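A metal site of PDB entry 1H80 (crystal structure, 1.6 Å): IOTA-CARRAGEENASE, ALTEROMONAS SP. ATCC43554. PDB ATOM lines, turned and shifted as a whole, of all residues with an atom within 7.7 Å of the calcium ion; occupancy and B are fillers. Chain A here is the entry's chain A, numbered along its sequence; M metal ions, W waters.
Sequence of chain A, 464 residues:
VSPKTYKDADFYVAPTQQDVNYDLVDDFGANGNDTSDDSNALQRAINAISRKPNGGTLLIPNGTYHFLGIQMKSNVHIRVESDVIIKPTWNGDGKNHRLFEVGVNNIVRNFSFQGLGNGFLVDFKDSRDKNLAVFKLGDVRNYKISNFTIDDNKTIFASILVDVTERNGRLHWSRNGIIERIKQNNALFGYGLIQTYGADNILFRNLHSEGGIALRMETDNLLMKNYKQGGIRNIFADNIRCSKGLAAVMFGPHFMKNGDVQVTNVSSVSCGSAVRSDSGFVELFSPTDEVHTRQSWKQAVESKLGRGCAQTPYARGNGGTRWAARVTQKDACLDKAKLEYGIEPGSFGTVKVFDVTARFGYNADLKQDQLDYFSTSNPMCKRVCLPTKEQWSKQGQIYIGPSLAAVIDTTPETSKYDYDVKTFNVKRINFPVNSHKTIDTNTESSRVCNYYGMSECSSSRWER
The backbone NH (N) of Thr 411 sits at hydrogen-bond distance from the side-chain carboxylate (OD1) of Asp 409 (2.9 Å).
The calcium ion is bound by O of Tyr 419, OD1 of Asp 420, OG1 of Thr 411, water W1, OD2 of Asp 418 and OD1 of Asp 418. The calcium ion has six donor atoms within binding distance.
Within 4 Å of the calcium ion: Thr 411, Asp 418, Tyr 419 and Asp 420. Along chain A the residues within 4 Å of the calcium ion span positions 411 to 420.
Water W1 bridges OD2 of Asp 409 (2.7 Å) and N of Val 421 (3.5 Å).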
ATOM      1  N   SER A 277      -1.304  19.452  -4.829  1.00  0.00           N
ATOM      2  CA  SER A 277      -2.380  19.660  -5.788  1.00  0.00           C
ATOM      3  C   SER A 277      -3.336  20.708  -5.226  1.00  0.00           C
ATOM      4  O   SER A 277      -3.838  20.570  -4.114  1.00  0.00           O
ATOM      5  CB  SER A 277      -3.125  18.349  -6.048  1.00  0.00           C
ATOM      6  OG  SER A 277      -2.248  17.393  -6.629  1.00  0.00           O
ATOM      7  N   ASP A 409      -3.031  17.809  -0.821  1.00  0.00           N
ATOM      8  CA  ASP A 409      -4.077  17.783  -1.833  1.00  0.00           C
ATOM      9  C   ASP A 409      -5.244  18.600  -1.311  1.00  0.00           C
ATOM     10  O   ASP A 409      -6.003  18.132  -0.462  1.00  0.00           O
ATOM     11  CB  ASP A 409      -4.545  16.350  -2.082  1.00  0.00           C
ATOM     12  CG  ASP A 409      -5.573  16.256  -3.191  1.00  0.00           C
ATOM     13  OD1 ASP A 409      -6.332  17.229  -3.388  1.00  0.00           O
ATOM     14  OD2 ASP A 409      -5.632  15.206  -3.875  1.00  0.00           O
ATOM     15  N   THR A 410      -5.387  19.824  -1.824  1.00  0.00           N
ATOM     16  CA  THR A 410      -6.464  20.690  -1.391  1.00  0.00           C
ATOM     17  C   THR A 410      -7.611  20.765  -2.399  1.00  0.00           C
ATOM     18  O   THR A 410      -8.335  21.759  -2.444  1.00  0.00           O
ATOM     19  CB  THR A 410      -5.960  22.112  -1.079  1.00  0.00           C
ATOM     20  OG1 THR A 410      -5.308  22.657  -2.232  1.00  0.00           O
ATOM     21  CG2 THR A 410      -4.975  22.087   0.089  1.00  0.00           C
ATOM     22  N   THR A 411      -7.759  19.727  -3.217  1.00  0.00           N
ATOM     23  CA  THR A 411      -8.842  19.698  -4.184  1.00  0.00           C
ATOM     24  C   THR A 411     -10.099  19.302  -3.405  1.00  0.00           C
ATOM     25  O   THR A 411     -10.046  18.459  -2.511  1.00  0.00           O
ATOM     26  CB  THR A 411      -8.593  18.674  -5.313  1.00  0.00           C
ATOM     27  OG1 THR A 411      -8.478  17.361  -4.768  1.00  0.00           O
ATOM     28  CG2 THR A 411      -7.315  19.030  -6.069  1.00  0.00           C
ATOM     29  N   PRO A 412     -11.246  19.898  -3.741  1.00  0.00           N
ATOM     30  CA  PRO A 412     -12.519  19.599  -3.066  1.00  0.00           C
ATOM     31  C   PRO A 412     -13.079  18.211  -3.347  1.00  0.00           C
ATOM     32  O   PRO A 412     -13.792  18.012  -4.329  1.00  0.00           O
ATOM     33  CB  PRO A 412     -13.437  20.710  -3.573  1.00  0.00           C
ATOM     34  CG  PRO A 412     -12.958  20.890  -4.985  1.00  0.00           C
ATOM     35  CD  PRO A 412     -11.453  20.890  -4.821  1.00  0.00           C
ATOM     36  N   GLU A 413     -12.758  17.256  -2.468  1.00  0.00           N
ATOM     37  CA  GLU A 413     -13.228  15.887  -2.615  1.00  0.00           C
ATOM     38  C   GLU A 413     -14.735  15.797  -2.824  1.00  0.00           C
ATOM     39  O   GLU A 413     -15.210  15.001  -3.636  1.00  0.00           O
ATOM     40  CB  GLU A 413     -12.832  15.059  -1.379  1.00  0.00           C
ATOM     41  N   THR A 414     -15.479  16.615  -2.081  1.00  0.00           N
ATOM     42  CA  THR A 414     -16.934  16.618  -2.182  1.00  0.00           C
ATOM     43  C   THR A 414     -17.401  17.741  -3.107  1.00  0.00           C
ATOM     44  O   THR A 414     -17.938  18.747  -2.651  1.00  0.00           O
ATOM     45  CB  THR A 414     -17.587  16.824  -0.805  1.00  0.00           C
ATOM     46  N   SER A 415     -17.197  17.567  -4.407  1.00  0.00           N
ATOM     47  CA  SER A 415     -17.616  18.590  -5.363  1.00  0.00           C
ATOM     48  C   SER A 415     -17.743  18.048  -6.783  1.00  0.00           C
ATOM     49  O   SER A 415     -17.035  17.119  -7.176  1.00  0.00           O
ATOM     50  CB  SER A 415     -16.621  19.749  -5.351  1.00  0.00           C
ATOM     51  OG  SER A 415     -16.950  20.713  -6.346  1.00  0.00           O
ATOM     52  N   TYR A 417     -17.064  19.850  -9.159  1.00  0.00           N
ATOM     53  CA  TYR A 417     -15.904  20.465  -9.770  1.00  0.00           C
ATOM     54  C   TYR A 417     -14.688  20.034  -8.960  1.00  0.00           C
ATOM     55  O   TYR A 417     -14.292  20.708  -8.001  1.00  0.00           O
ATOM     56  CB  TYR A 417     -16.012  21.984  -9.738  1.00  0.00           C
ATOM     57  CG  TYR A 417     -17.285  22.528 -10.342  1.00  0.00           C
ATOM     58  CD1 TYR A 417     -18.462  22.590  -9.597  1.00  0.00           C
ATOM     59  CD2 TYR A 417     -17.312  22.988 -11.655  1.00  0.00           C
ATOM     60  CE1 TYR A 417     -19.639  23.099 -10.156  1.00  0.00           C
ATOM     61  CE2 TYR A 417     -18.476  23.497 -12.219  1.00  0.00           C
ATOM     62  CZ  TYR A 417     -19.635  23.539 -11.465  1.00  0.00           C
ATOM     63  OH  TYR A 417     -20.796  24.044 -12.019  1.00  0.00           O
ATOM     64  N   ASP A 418     -14.105  18.914  -9.340  1.00  0.00           N
ATOM     65  CA  ASP A 418     -12.944  18.393  -8.647  1.00  0.00           C
ATOM     66  C   ASP A 418     -12.184  17.450  -9.564  1.00  0.00           C
ATOM     67  O   ASP A 418     -12.756  16.889 -10.503  1.00  0.00           O
ATOM     68  CB  ASP A 418     -13.383  17.631  -7.398  1.00  0.00           C
ATOM     69  CG  ASP A 418     -12.225  17.007  -6.642  1.00  0.00           C
ATOM     70  OD1 ASP A 418     -11.285  17.738  -6.270  1.00  0.00           O
ATOM     71  OD2 ASP A 418     -12.256  15.772  -6.411  1.00  0.00           O
ATOM     72  N   TYR A 419     -10.894  17.301  -9.320  1.00  0.00           N
ATOM     73  CA  TYR A 419     -10.083  16.392 -10.107  1.00  0.00           C
ATOM     74  C   TYR A 419      -9.262  15.622  -9.097  1.00  0.00           C
ATOM     75  O   TYR A 419      -9.100  16.062  -7.949  1.00  0.00           O
ATOM     76  CB  TYR A 419      -9.194  17.137 -11.117  1.00  0.00           C
ATOM     77  CG  TYR A 419      -8.087  17.966 -10.517  1.00  0.00           C
ATOM     78  CD1 TYR A 419      -8.312  19.253 -10.033  1.00  0.00           C
ATOM     79  CD2 TYR A 419      -6.785  17.466 -10.440  1.00  0.00           C
ATOM     80  CE1 TYR A 419      -7.287  20.024  -9.495  1.00  0.00           C
ATOM     81  CE2 TYR A 419      -5.749  18.210  -9.916  1.00  0.00           C
ATOM     82  CZ  TYR A 419      -6.006  19.487  -9.437  1.00  0.00           C
ATOM     83  OH  TYR A 419      -4.972  20.218  -8.894  1.00  0.00           O
ATOM     84  N   ASP A 420      -8.755  14.467  -9.499  1.00  0.00           N
ATOM     85  CA  ASP A 420      -7.978  13.657  -8.578  1.00  0.00           C
ATOM     86  C   ASP A 420      -6.568  13.369  -9.026  1.00  0.00           C
ATOM     87  O   ASP A 420      -6.312  13.011 -10.176  1.00  0.00           O
ATOM     88  CB  ASP A 420      -8.681  12.328  -8.302  1.00  0.00           C
ATOM     89  CG  ASP A 420     -10.076  12.507  -7.733  1.00  0.00           C
ATOM     90  OD1 ASP A 420     -10.252  13.339  -6.822  1.00  0.00           O
ATOM     91  OD2 ASP A 420     -10.983  11.798  -8.208  1.00  0.00           O
ATOM     92  N   VAL A 421      -5.633  13.540  -8.092  1.00  0.00           N
ATOM     93  CA  VAL A 421      -4.234  13.249  -8.347  1.00  0.00           C
ATOM     94  C   VAL A 421      -4.005  12.003  -7.503  1.00  0.00           C
ATOM     95  O   VAL A 421      -3.835  12.096  -6.286  1.00  0.00           O
ATOM     96  CB  VAL A 421      -3.321  14.395  -7.879  1.00  0.00           C
ATOM     97  CG1 VAL A 421      -1.871  13.985  -7.995  1.00  0.00           C
ATOM     98  CG2 VAL A 421      -3.590  15.643  -8.710  1.00  0.00           C
ATOM     99  N   THR A 441      -8.431  18.253   2.499  1.00  0.00           N
ATOM    100  CA  THR A 441      -9.459  19.155   2.985  1.00  0.00           C
ATOM    101  C   THR A 441     -10.037  18.753   4.335  1.00  0.00           C
ATOM    102  O   THR A 441     -10.671  19.565   5.007  1.00  0.00           O
ATOM    103  CB  THR A 441     -10.616  19.257   1.968  1.00  0.00           C
ATOM    104  OG1 THR A 441     -11.197  17.970   1.775  1.00  0.00           O
ATOM    105  CG2 THR A 441     -10.098  19.774   0.635  1.00  0.00           C
HETATM  106 CA    CA M   1      -9.807  15.487  -5.709  1.00  0.00          CA
HETATM  107  O   HOH W   1      -7.641  14.246  -5.315  1.00  0.00           O
